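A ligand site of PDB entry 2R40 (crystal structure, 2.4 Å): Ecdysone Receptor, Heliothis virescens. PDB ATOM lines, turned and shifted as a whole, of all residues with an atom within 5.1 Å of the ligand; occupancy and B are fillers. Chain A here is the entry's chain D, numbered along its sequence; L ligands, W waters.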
ATOM      1  N   GLU A  43     -11.297 -17.442 -28.904  1.00  0.00           N
ATOM      2  CA  GLU A  43     -10.374 -17.572 -27.779  1.00  0.00           C
ATOM      3  C   GLU A  43      -9.618 -18.896 -27.789  1.00  0.00           C
ATOM      4  O   GLU A  43      -8.568 -19.042 -27.165  1.00  0.00           O
ATOM      5  CB  GLU A  43     -11.096 -17.328 -26.453  1.00  0.00           C
ATOM      6  CG  GLU A  43     -10.202 -16.670 -25.361  1.00  0.00           C
ATOM      7  CD  GLU A  43      -9.613 -15.300 -25.736  1.00  0.00           C
ATOM      8  OE1 GLU A  43      -9.714 -14.824 -26.904  1.00  0.00           O
ATOM      9  OE2 GLU A  43      -9.005 -14.689 -24.836  1.00  0.00           O
ATOM     10  N   GLN A  44     -10.172 -19.858 -28.529  1.00  0.00           N
ATOM     11  CA  GLN A  44      -9.531 -21.141 -28.727  1.00  0.00           C
ATOM     12  C   GLN A  44      -9.535 -21.486 -30.194  1.00  0.00           C
ATOM     13  O   GLN A  44     -10.471 -21.104 -30.916  1.00  0.00           O
ATOM     14  CB  GLN A  44     -10.276 -22.237 -27.965  1.00  0.00           C
ATOM     15  CG  GLN A  44      -9.832 -22.390 -26.533  1.00  0.00           C
ATOM     16  CD  GLN A  44     -10.590 -23.486 -25.815  1.00  0.00           C
ATOM     17  OE1 GLN A  44     -10.213 -23.899 -24.717  1.00  0.00           O
ATOM     18  NE2 GLN A  44     -11.669 -23.968 -26.424  1.00  0.00           N
ATOM     19  N   PRO A  45      -8.505 -22.215 -30.657  1.00  0.00           N
ATOM     20  CA  PRO A  45      -8.490 -22.690 -32.038  1.00  0.00           C
ATOM     21  C   PRO A  45      -9.616 -23.678 -32.297  1.00  0.00           C
ATOM     22  O   PRO A  45     -10.080 -24.345 -31.378  1.00  0.00           O
ATOM     23  CB  PRO A  45      -7.128 -23.386 -32.175  1.00  0.00           C
ATOM     24  CG  PRO A  45      -6.639 -23.606 -30.808  1.00  0.00           C
ATOM     25  CD  PRO A  45      -7.299 -22.599 -29.911  1.00  0.00           C
ATOM     26  N   ILE A  73       4.679 -25.271 -28.230  1.00  0.00           N
ATOM     27  CA  ILE A  73       4.726 -23.829 -27.956  1.00  0.00           C
ATOM     28  C   ILE A  73       4.700 -22.986 -29.254  1.00  0.00           C
ATOM     29  O   ILE A  73       3.863 -22.092 -29.392  1.00  0.00           O
ATOM     30  CB  ILE A  73       5.967 -23.454 -27.065  1.00  0.00           C
ATOM     31  CG1 ILE A  73       5.750 -23.952 -25.642  1.00  0.00           C
ATOM     32  CG2 ILE A  73       6.215 -21.945 -27.070  1.00  0.00           C
ATOM     33  CD1 ILE A  73       6.859 -23.642 -24.643  1.00  0.00           C
ATOM     34  N   THR A  74       5.600 -23.281 -30.178  1.00  0.00           N
ATOM     35  CA  THR A  74       5.666 -22.559 -31.452  1.00  0.00           C
ATOM     36  C   THR A  74       4.429 -22.783 -32.331  1.00  0.00           C
ATOM     37  O   THR A  74       3.875 -21.814 -32.845  1.00  0.00           O
ATOM     38  CB  THR A  74       6.984 -22.815 -32.233  1.00  0.00           C
ATOM     39  OG1 THR A  74       7.068 -24.192 -32.616  1.00  0.00           O
ATOM     40  CG2 THR A  74       8.214 -22.439 -31.401  1.00  0.00           C
ATOM     41  N   MET A  76       1.323 -23.808 -31.342  1.00  0.00           N
ATOM     42  CA  MET A  76       0.161 -23.150 -30.722  1.00  0.00           C
ATOM     43  C   MET A  76       0.200 -21.630 -30.871  1.00  0.00           C
ATOM     44  O   MET A  76      -0.842 -20.992 -30.958  1.00  0.00           O
ATOM     45  CB  MET A  76       0.017 -23.491 -29.229  1.00  0.00           C
ATOM     46  CG  MET A  76      -0.353 -24.939 -28.920  1.00  0.00           C
ATOM     47  SD  MET A  76      -1.785 -25.608 -29.775  1.00  0.00           S
ATOM     48  CE  MET A  76      -3.021 -24.342 -29.447  1.00  0.00           C
ATOM     49  N   THR A  77       1.407 -21.050 -30.897  1.00  0.00           N
ATOM     50  CA  THR A  77       1.596 -19.602 -31.084  1.00  0.00           C
ATOM     51  C   THR A  77       1.197 -19.154 -32.481  1.00  0.00           C
ATOM     52  O   THR A  77       0.661 -18.082 -32.643  1.00  0.00           O
ATOM     53  CB  THR A  77       3.044 -19.142 -30.734  1.00  0.00           C
ATOM     54  OG1 THR A  77       3.330 -19.523 -29.395  1.00  0.00           O
ATOM     55  CG2 THR A  77       3.184 -17.616 -30.850  1.00  0.00           C
ATOM     56  N   THR A  80      -2.614 -19.143 -32.183  1.00  0.00           N
ATOM     57  CA  THR A  80      -3.013 -17.974 -31.395  1.00  0.00           C
ATOM     58  C   THR A  80      -2.983 -16.705 -32.248  1.00  0.00           C
ATOM     59  O   THR A  80      -3.943 -15.931 -32.216  1.00  0.00           O
ATOM     60  CB  THR A  80      -2.059 -17.785 -30.201  1.00  0.00           C
ATOM     61  OG1 THR A  80      -2.093 -18.969 -29.399  1.00  0.00           O
ATOM     62  CG2 THR A  80      -2.443 -16.587 -29.345  1.00  0.00           C
ATOM     63  N   LEU A  83      -5.779 -16.403 -34.645  1.00  0.00           N
ATOM     64  CA  LEU A  83      -7.021 -16.062 -33.935  1.00  0.00           C
ATOM     65  C   LEU A  83      -7.102 -14.541 -33.663  1.00  0.00           C
ATOM     66  O   LEU A  83      -8.183 -13.939 -33.765  1.00  0.00           O
ATOM     67  CB  LEU A  83      -7.065 -16.832 -32.619  1.00  0.00           C
ATOM     68  CG  LEU A  83      -7.827 -18.123 -32.265  1.00  0.00           C
ATOM     69  CD1 LEU A  83      -8.589 -18.837 -33.375  1.00  0.00           C
ATOM     70  CD2 LEU A  83      -6.939 -19.071 -31.433  1.00  0.00           C
ATOM     71  N   MET A 114      -1.389 -11.236 -27.264  1.00  0.00           N
ATOM     72  CA  MET A 114      -1.099 -12.609 -26.896  1.00  0.00           C
ATOM     73  C   MET A 114      -0.877 -12.719 -25.373  1.00  0.00           C
ATOM     74  O   MET A 114      -1.167 -13.753 -24.789  1.00  0.00           O
ATOM     75  CB  MET A 114       0.121 -13.084 -27.689  1.00  0.00           C
ATOM     76  CG  MET A 114       0.626 -14.477 -27.397  1.00  0.00           C
ATOM     77  SD  MET A 114       1.815 -15.049 -28.637  1.00  0.00           S
ATOM     78  CE  MET A 114       3.238 -14.027 -28.292  1.00  0.00           C
ATOM     79  N   MET A 115      -0.380 -11.650 -24.767  1.00  0.00           N
ATOM     80  CA  MET A 115      -0.132 -11.597 -23.321  1.00  0.00           C
ATOM     81  C   MET A 115      -1.418 -11.558 -22.503  1.00  0.00           C
ATOM     82  O   MET A 115      -1.452 -12.046 -21.372  1.00  0.00           O
ATOM     83  CB  MET A 115       0.746 -10.388 -22.976  1.00  0.00           C
ATOM     84  CG  MET A 115       2.090 -10.361 -23.647  1.00  0.00           C
ATOM     85  SD  MET A 115       2.995 -11.912 -23.513  1.00  0.00           S
ATOM     86  CE  MET A 115       4.054 -11.775 -24.945  1.00  0.00           C
ATOM     87  N   ARG A 117      -4.241 -12.935 -23.598  1.00  0.00           N
ATOM     88  CA  ARG A 117      -4.751 -14.289 -23.819  1.00  0.00           C
ATOM     89  C   ARG A 117      -4.135 -15.358 -22.891  1.00  0.00           C
ATOM     90  O   ARG A 117      -4.826 -16.299 -22.511  1.00  0.00           O
ATOM     91  CB  ARG A 117      -4.650 -14.699 -25.315  1.00  0.00           C
ATOM     92  CG  ARG A 117      -5.447 -13.737 -26.235  1.00  0.00           C
ATOM     93  CD  ARG A 117      -5.262 -13.996 -27.739  1.00  0.00           C
ATOM     94  NE  ARG A 117      -5.892 -15.246 -28.102  1.00  0.00           N
ATOM     95  CZ  ARG A 117      -6.952 -15.393 -28.905  1.00  0.00           C
ATOM     96  NH1 ARG A 117      -7.517 -14.363 -29.516  1.00  0.00           N
ATOM     97  NH2 ARG A 117      -7.410 -16.596 -29.109  1.00  0.00           N
ATOM     98  N   VAL A 118      -2.861 -15.229 -22.536  1.00  0.00           N
ATOM     99  CA  VAL A 118      -2.250 -16.167 -21.585  1.00  0.00           C
ATOM    100  C   VAL A 118      -2.703 -15.858 -20.151  1.00  0.00           C
ATOM    101  O   VAL A 118      -2.912 -16.778 -19.350  1.00  0.00           O
ATOM    102  CB  VAL A 118      -0.687 -16.227 -21.717  1.00  0.00           C
ATOM    103  CG1 VAL A 118      -0.105 -14.869 -21.786  1.00  0.00           C
ATOM    104  CG2 VAL A 118      -0.045 -16.953 -20.547  1.00  0.00           C
ATOM    105  N   ARG A 121      -5.713 -17.645 -19.221  1.00  0.00           N
ATOM    106  CA  ARG A 121      -5.506 -19.099 -19.146  1.00  0.00           C
ATOM    107  C   ARG A 121      -4.545 -19.508 -18.031  1.00  0.00           C
ATOM    108  O   ARG A 121      -4.063 -20.653 -17.980  1.00  0.00           O
ATOM    109  CB  ARG A 121      -4.934 -19.606 -20.480  1.00  0.00           C
ATOM    110  CG  ARG A 121      -5.788 -19.395 -21.712  1.00  0.00           C
ATOM    111  CD  ARG A 121      -7.265 -19.733 -21.521  1.00  0.00           C
ATOM    112  NE  ARG A 121      -7.583 -21.124 -21.238  1.00  0.00           N
ATOM    113  CZ  ARG A 121      -7.383 -22.169 -22.047  1.00  0.00           C
ATOM    114  NH1 ARG A 121      -6.785 -22.011 -23.244  1.00  0.00           N
ATOM    115  NH2 ARG A 121      -7.749 -23.388 -21.650  1.00  0.00           N
ATOM    116  N   VAL A 129       0.287 -22.160 -17.184  1.00  0.00           N
ATOM    117  CA  VAL A 129      -0.569 -21.722 -18.285  1.00  0.00           C
ATOM    118  C   VAL A 129      -1.291 -22.952 -18.835  1.00  0.00           C
ATOM    119  O   VAL A 129      -0.678 -23.997 -19.076  1.00  0.00           O
ATOM    120  CB  VAL A 129       0.241 -21.016 -19.418  1.00  0.00           C
ATOM    121  CG1 VAL A 129      -0.685 -20.513 -20.529  1.00  0.00           C
ATOM    122  CG2 VAL A 129       1.075 -19.861 -18.838  1.00  0.00           C
ATOM    123  N   LEU A 130      -2.598 -22.813 -19.018  1.00  0.00           N
ATOM    124  CA  LEU A 130      -3.406 -23.899 -19.532  1.00  0.00           C
ATOM    125  C   LEU A 130      -3.522 -23.726 -21.053  1.00  0.00           C
ATOM    126  O   LEU A 130      -4.061 -22.734 -21.542  1.00  0.00           O
ATOM    127  CB  LEU A 130      -4.774 -23.934 -18.807  1.00  0.00           C
ATOM    128  CG  LEU A 130      -4.680 -23.846 -17.270  1.00  0.00           C
ATOM    129  CD1 LEU A 130      -6.056 -23.624 -16.541  1.00  0.00           C
ATOM    130  CD2 LEU A 130      -3.918 -25.041 -16.656  1.00  0.00           C
ATOM    131  N   PHE A 131      -2.967 -24.696 -21.788  1.00  0.00           N
ATOM    132  CA  PHE A 131      -2.994 -24.657 -23.251  1.00  0.00           C
ATOM    133  C   PHE A 131      -4.334 -25.166 -23.770  1.00  0.00           C
ATOM    134  O   PHE A 131      -5.096 -25.782 -23.003  1.00  0.00           O
ATOM    135  CB  PHE A 131      -1.813 -25.459 -23.844  1.00  0.00           C
ATOM    136  CG  PHE A 131      -0.493 -24.724 -23.832  1.00  0.00           C
ATOM    137  CD1 PHE A 131      -0.255 -23.675 -22.936  1.00  0.00           C
ATOM    138  CD2 PHE A 131       0.528 -25.102 -24.699  1.00  0.00           C
ATOM    139  CE1 PHE A 131       0.971 -23.010 -22.911  1.00  0.00           C
ATOM    140  CE2 PHE A 131       1.762 -24.439 -24.694  1.00  0.00           C
ATOM    141  CZ  PHE A 131       1.983 -23.392 -23.801  1.00  0.00           C
ATOM    142  N   ALA A 132      -4.635 -24.910 -25.035  1.00  0.00           N
ATOM    143  CA  ALA A 132      -5.946 -25.227 -25.608  1.00  0.00           C
ATOM    144  C   ALA A 132      -6.293 -26.720 -25.550  1.00  0.00           C
ATOM    145  O   ALA A 132      -7.469 -27.095 -25.519  1.00  0.00           O
ATOM    146  CB  ALA A 132      -6.082 -24.683 -27.026  1.00  0.00           C
ATOM    147  N   ASN A 133      -5.263 -27.567 -25.507  1.00  0.00           N
ATOM    148  CA  ASN A 133      -5.417 -29.001 -25.287  1.00  0.00           C
ATOM    149  C   ASN A 133      -5.641 -29.402 -23.814  1.00  0.00           C
ATOM    150  O   ASN A 133      -5.756 -30.579 -23.506  1.00  0.00           O
ATOM    151  CB  ASN A 133      -4.193 -29.750 -25.836  1.00  0.00           C
ATOM    152  CG  ASN A 133      -2.901 -29.424 -25.085  1.00  0.00           C
ATOM    153  OD1 ASN A 133      -2.767 -28.376 -24.430  1.00  0.00           O
ATOM    154  ND2 ASN A 133      -1.933 -30.327 -25.168  1.00  0.00           N
ATOM    155  N   TYR A 142       8.843 -24.595 -20.303  1.00  0.00           N
ATOM    156  CA  TYR A 142       9.415 -23.508 -21.086  1.00  0.00           C
ATOM    157  C   TYR A 142      10.928 -23.545 -21.036  1.00  0.00           C
ATOM    158  O   TYR A 142      11.597 -23.151 -21.994  1.00  0.00           O
ATOM    159  CB  TYR A 142       8.931 -22.146 -20.571  1.00  0.00           C
ATOM    160  CG  TYR A 142       7.580 -21.716 -21.081  1.00  0.00           C
ATOM    161  CD1 TYR A 142       6.402 -22.261 -20.556  1.00  0.00           C
ATOM    162  CD2 TYR A 142       7.468 -20.717 -22.084  1.00  0.00           C
ATOM    163  CE1 TYR A 142       5.166 -21.877 -21.013  1.00  0.00           C
ATOM    164  CE2 TYR A 142       6.212 -20.325 -22.535  1.00  0.00           C
ATOM    165  CZ  TYR A 142       5.063 -20.907 -21.996  1.00  0.00           C
ATOM    166  OH  TYR A 142       3.814 -20.531 -22.433  1.00  0.00           O
ATOM    167  N   MET A 147      12.987 -21.596 -23.612  1.00  0.00           N
ATOM    168  CA  MET A 147      12.337 -20.291 -23.478  1.00  0.00           C
ATOM    169  C   MET A 147      12.208 -19.817 -22.038  1.00  0.00           C
ATOM    170  O   MET A 147      11.242 -19.136 -21.686  1.00  0.00           O
ATOM    171  CB  MET A 147      10.992 -20.299 -24.204  1.00  0.00           C
ATOM    172  CG  MET A 147      11.139 -20.668 -25.662  1.00  0.00           C
ATOM    173  SD  MET A 147       9.614 -20.500 -26.546  1.00  0.00           S
ATOM    174  CE  MET A 147       9.939 -21.521 -27.996  1.00  0.00           C
ATOM    175  N   VAL A 150      11.749 -15.993 -21.142  1.00  0.00           N
ATOM    176  CA  VAL A 150      10.486 -15.325 -21.317  1.00  0.00           C
ATOM    177  C   VAL A 150       9.454 -15.612 -20.186  1.00  0.00           C
ATOM    178  O   VAL A 150       8.615 -14.762 -19.878  1.00  0.00           O
ATOM    179  CB  VAL A 150       9.959 -15.630 -22.748  1.00  0.00           C
ATOM    180  CG1 VAL A 150       8.638 -16.385 -22.769  1.00  0.00           C
ATOM    181  CG2 VAL A 150       9.934 -14.346 -23.607  1.00  0.00           C
ATOM    182  N   LEU A 154       6.440 -13.275 -17.701  1.00  0.00           N
ATOM    183  CA  LEU A 154       5.126 -13.649 -18.164  1.00  0.00           C
ATOM    184  C   LEU A 154       4.219 -14.137 -17.019  1.00  0.00           C
ATOM    185  O   LEU A 154       3.082 -13.710 -16.933  1.00  0.00           O
ATOM    186  CB  LEU A 154       5.240 -14.696 -19.269  1.00  0.00           C
ATOM    187  CG  LEU A 154       3.970 -15.156 -19.991  1.00  0.00           C
ATOM    188  CD1 LEU A 154       3.118 -13.974 -20.452  1.00  0.00           C
ATOM    189  CD2 LEU A 154       4.373 -16.046 -21.187  1.00  0.00           C
ATOM    190  N   ASN A 238       9.253 -10.852 -26.107  1.00  0.00           N
ATOM    191  CA  ASN A 238       8.874 -11.823 -27.128  1.00  0.00           C
ATOM    192  C   ASN A 238       9.701 -11.690 -28.414  1.00  0.00           C
ATOM    193  O   ASN A 238      10.130 -12.701 -28.981  1.00  0.00           O
ATOM    194  CB  ASN A 238       7.377 -11.782 -27.439  1.00  0.00           C
ATOM    195  CG  ASN A 238       6.953 -12.847 -28.443  1.00  0.00           C
ATOM    196  OD1 ASN A 238       6.940 -14.024 -28.131  1.00  0.00           O
ATOM    197  ND2 ASN A 238       6.637 -12.424 -29.662  1.00  0.00           N
ATOM    198  N   MET A 241      13.289 -12.964 -27.660  1.00  0.00           N
ATOM    199  CA  MET A 241      13.248 -14.404 -27.619  1.00  0.00           C
ATOM    200  C   MET A 241      13.332 -14.992 -29.037  1.00  0.00           C
ATOM    201  O   MET A 241      14.113 -15.924 -29.286  1.00  0.00           O
ATOM    202  CB  MET A 241      11.976 -14.885 -26.916  1.00  0.00           C
ATOM    203  CG  MET A 241      11.911 -16.388 -26.633  1.00  0.00           C
ATOM    204  SD  MET A 241      12.999 -16.925 -25.298  1.00  0.00           S
ATOM    205  CE  MET A 241      14.358 -17.693 -26.183  1.00  0.00           C
ATOM    206  N   CYS A 242      12.548 -14.432 -29.964  1.00  0.00           N
ATOM    207  CA  CYS A 242      12.539 -14.860 -31.359  1.00  0.00           C
ATOM    208  C   CYS A 242      13.884 -14.658 -32.032  1.00  0.00           C
ATOM    209  O   CYS A 242      14.361 -15.540 -32.748  1.00  0.00           O
ATOM    210  CB  CYS A 242      11.461 -14.119 -32.157  1.00  0.00           C
ATOM    211  SG  CYS A 242       9.811 -14.568 -31.701  1.00  0.00           S
ATOM    212  N   LEU A 245      16.357 -17.213 -30.549  1.00  0.00           N
ATOM    213  CA  LEU A 245      16.102 -18.536 -31.132  1.00  0.00           C
ATOM    214  C   LEU A 245      16.663 -18.686 -32.548  1.00  0.00           C
ATOM    215  O   LEU A 245      17.202 -19.742 -32.884  1.00  0.00           O
ATOM    216  CB  LEU A 245      14.596 -18.850 -31.120  1.00  0.00           C
ATOM    217  CG  LEU A 245      13.949 -19.159 -29.769  1.00  0.00           C
ATOM    218  CD1 LEU A 245      12.422 -18.983 -29.824  1.00  0.00           C
ATOM    219  CD2 LEU A 245      14.313 -20.550 -29.264  1.00  0.00           C
ATOM    220  N   LEU A 252      12.456 -21.960 -35.688  1.00  0.00           N
ATOM    221  CA  LEU A 252      11.378 -20.982 -35.556  1.00  0.00           C
ATOM    222  C   LEU A 252      10.594 -20.803 -36.867  1.00  0.00           C
ATOM    223  O   LEU A 252      11.159 -20.390 -37.871  1.00  0.00           O
ATOM    224  CB  LEU A 252      11.932 -19.637 -35.066  1.00  0.00           C
ATOM    225  CG  LEU A 252      11.036 -18.655 -34.284  1.00  0.00           C
ATOM    226  CD1 LEU A 252      10.103 -17.854 -35.189  1.00  0.00           C
ATOM    227  CD2 LEU A 252      10.247 -19.315 -33.145  1.00  0.00           C
ATOM    228  N   LEU A 256       5.895 -16.803 -37.972  1.00  0.00           N
ATOM    229  CA  LEU A 256       6.204 -16.008 -36.780  1.00  0.00           C
ATOM    230  C   LEU A 256       7.391 -15.063 -37.010  1.00  0.00           C
ATOM    231  O   LEU A 256       7.387 -13.920 -36.542  1.00  0.00           O
ATOM    232  CB  LEU A 256       6.470 -16.944 -35.597  1.00  0.00           C
ATOM    233  CG  LEU A 256       5.335 -17.278 -34.610  1.00  0.00           C
ATOM    234  CD1 LEU A 256       3.930 -16.906 -35.080  1.00  0.00           C
ATOM    235  CD2 LEU A 256       5.431 -18.720 -34.154  1.00  0.00           C
ATOM    236  N   TRP A 260       6.840 -10.949 -36.710  1.00  0.00           N
ATOM    237  CA  TRP A 260       7.640 -10.333 -35.660  1.00  0.00           C
ATOM    238  C   TRP A 260       9.016  -9.852 -36.109  1.00  0.00           C
ATOM    239  O   TRP A 260       9.870  -9.551 -35.283  1.00  0.00           O
ATOM    240  CB  TRP A 260       7.714 -11.254 -34.434  1.00  0.00           C
ATOM    241  CG  TRP A 260       6.364 -11.439 -33.803  1.00  0.00           C
ATOM    242  CD1 TRP A 260       5.317 -10.563 -33.846  1.00  0.00           C
ATOM    243  CD2 TRP A 260       5.916 -12.566 -33.052  1.00  0.00           C
ATOM    244  NE1 TRP A 260       4.244 -11.074 -33.171  1.00  0.00           N
ATOM    245  CE2 TRP A 260       4.582 -12.298 -32.665  1.00  0.00           C
ATOM    246  CE3 TRP A 260       6.511 -13.780 -32.665  1.00  0.00           C
ATOM    247  CZ2 TRP A 260       3.836 -13.206 -31.910  1.00  0.00           C
ATOM    248  CZ3 TRP A 260       5.766 -14.667 -31.902  1.00  0.00           C
ATOM    249  CH2 TRP A 260       4.439 -14.367 -31.533  1.00  0.00           C
HETATM  250  C1  LIG L   1      -2.894 -20.261 -23.826  1.00  0.00           C
HETATM  251  C2  LIG L   1      -3.151 -19.997 -25.307  1.00  0.00           C
HETATM  252  C3  LIG L   1      -4.291 -18.954 -25.390  1.00  0.00           C
HETATM  253  C4  LIG L   1      -4.710 -18.699 -26.847  1.00  0.00           C
HETATM  254  O1  LIG L   1      -5.796 -17.751 -26.881  1.00  0.00           O
HETATM  255  C5  LIG L   1      -5.106 -19.997 -27.565  1.00  0.00           C
HETATM  256  O2  LIG L   1      -6.332 -20.477 -27.041  1.00  0.00           O
HETATM  257  C6  LIG L   1      -4.048 -21.109 -27.438  1.00  0.00           C
HETATM  258  C7  LIG L   1      -3.546 -21.322 -25.998  1.00  0.00           C
HETATM  259  C8  LIG L   1      -2.365 -22.299 -26.154  1.00  0.00           C
HETATM  260  O3  LIG L   1      -2.611 -23.511 -26.242  1.00  0.00           O
HETATM  261  C9  LIG L   1      -1.057 -21.826 -26.291  1.00  0.00           C
HETATM  262  C10 LIG L   1      -0.740 -20.458 -26.212  1.00  0.00           C
HETATM  263  C11 LIG L   1      -1.870 -19.397 -26.029  1.00  0.00           C
HETATM  264  C12 LIG L   1      -1.347 -18.057 -25.386  1.00  0.00           C
HETATM  265  C13 LIG L   1       0.138 -17.673 -25.709  1.00  0.00           C
HETATM  266  C14 LIG L   1       1.113 -18.821 -25.431  1.00  0.00           C
HETATM  267  C15 LIG L   1       1.048 -19.242 -23.927  1.00  0.00           C
HETATM  268  C16 LIG L   1       0.716 -19.957 -26.394  1.00  0.00           C
HETATM  269  O4  LIG L   1       0.756 -19.478 -27.746  1.00  0.00           O
HETATM  270  C17 LIG L   1       1.861 -20.944 -26.248  1.00  0.00           C
HETATM  271  C18 LIG L   1       3.101 -20.029 -26.161  1.00  0.00           C
HETATM  272  C19 LIG L   1       2.593 -18.580 -25.921  1.00  0.00           C
HETATM  273  C20 LIG L   1       3.616 -17.697 -25.062  1.00  0.00           C
HETATM  274  O5  LIG L   1       3.620 -18.076 -23.697  1.00  0.00           O
HETATM  275  C21 LIG L   1       3.244 -16.213 -25.053  1.00  0.00           C
HETATM  276  C22 LIG L   1       5.101 -17.882 -25.590  1.00  0.00           C
HETATM  277  O6  LIG L   1       6.080 -17.273 -24.676  1.00  0.00           O
HETATM  278  C23 LIG L   1       5.367 -17.402 -27.044  1.00  0.00           C
HETATM  279  C24 LIG L   1       6.901 -17.418 -27.333  1.00  0.00           C
HETATM  280  C25 LIG L   1       7.272 -17.266 -28.828  1.00  0.00           C
HETATM  281  C26 LIG L   1       7.008 -18.573 -29.595  1.00  0.00           C
HETATM  282  C27 LIG L   1       8.749 -16.874 -28.915  1.00  0.00           C
HETATM  283  O7  LIG L   1       6.468 -16.222 -29.401  1.00  0.00           O
HETATM  284  O   HOH W   1       6.491 -14.565 -25.174  1.00  0.00           O
HETATM  285  O   HOH W   2      -6.913 -17.146 -23.769  1.00  0.00           O
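Gln 44 touches the ligand. Pro 45 touches the ligand. Ile 73 touches the ligand (CG2 to C18, 3.8 Å). CE of Met 76 touches O3 of the ligand, at 3.3 Å. Met 114 touches the ligand. Arg 121 touches the ligand (CG to C1, 3.7 Å). Val 129 touches the ligand (CG1 to C1, 3.98 Å). O of Leu 130 touches C1 of the ligand, 3.6 Å away. Phe 131 touches the ligand (CB to O3, 3.2 Å). Val 150 touches the ligand. CD2 of Leu 154 touches O5 of the ligand (3.3 Å). Met 241 touches the ligand. Cys 242 touches the ligand. CZ3 of Trp 260 touches O7 of the ligand, at 3.0 Å. Hydrophobic or aromatic side chains within 4 Å of the ligand: Pro 45, Ile 73, Met 76, Met 114, Val 129, Phe 131, Ala 132, Tyr 142, Val 150, Leu 154, Met 241 and Trp 260. Within 4 Å of the ligand: Glu 43, Gln 44, Pro 45, Ile 73, Met 76, Thr 77, Thr 80, Met 114, Arg 117, Arg 121, Val 129, Leu 130, Phe 131, Ala 132, Tyr 142, Val 150, Leu 154, Asn 238, Met 241, Cys 242 and Trp 260.
The side-chain sulfur (SG) of Cys 242 sits at hydrogen-bond distance from the backbone carbonyl oxygen (O) of Asn 238 (3.3 Å). NH1 of Arg 117 lies within salt-bridge range of OE1 of Glu 43. The backbone carbonyl oxygen (O) of Tyr 142 sits at hydrogen-bond distance from the backbone NH (N) of Met 147, 2.6 Å away. OG1 of Thr 77 lies within hydrogen-bond range of O of Ile 73, 2.6 Å away. The side-chain hydroxyl (OG1) of Thr 80 is in hydrogen-bond range of the backbone carbonyl oxygen (O) of Met 76 (2.8 Å). O of Arg 121 lies within hydrogen-bond range of N of Leu 130 (2.8 Å).
The side-chain amide oxygen of Asn 238 is in hydrogen-bond range of an oxygen (O7) of the ligand (2.6 Å). O of Glu 43 lies within hydrogen-bond range of O2 of the ligand (2.7 Å). The backbone NH of Ala 132 lies within hydrogen-bond range of an oxygen (O3) of the ligand, at 2.7 Å. An oxygen (O5) of the ligand lies within hydrogen-bond range of the side-chain hydroxyl (OH) of Tyr 142, 2.8 Å away. An oxygen (O1) of the ligand sits at hydrogen-bond distance from the guanidinium group (NE) of Arg 117, 2.8 Å away. O4 of the ligand sits at hydrogen-bond distance from OG1 of Thr 77 (3.1 Å). The side-chain hydroxyl (OG1) of Thr 80 lies within hydrogen-bond range of an oxygen (O4) of the ligand (3.3 Å).
Water W1 bridges an oxygen (O6) of the ligand (2.8 Å) and the side-chain amide oxygen (OD1) of Asn 238 (3.0 Å). Water W2 lies within hydrogen-bond range of O of Arg 117 (2.6 Å), O1 of the ligand (3.4 Å) and OE2 of Glu 43 (3.4 Å).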
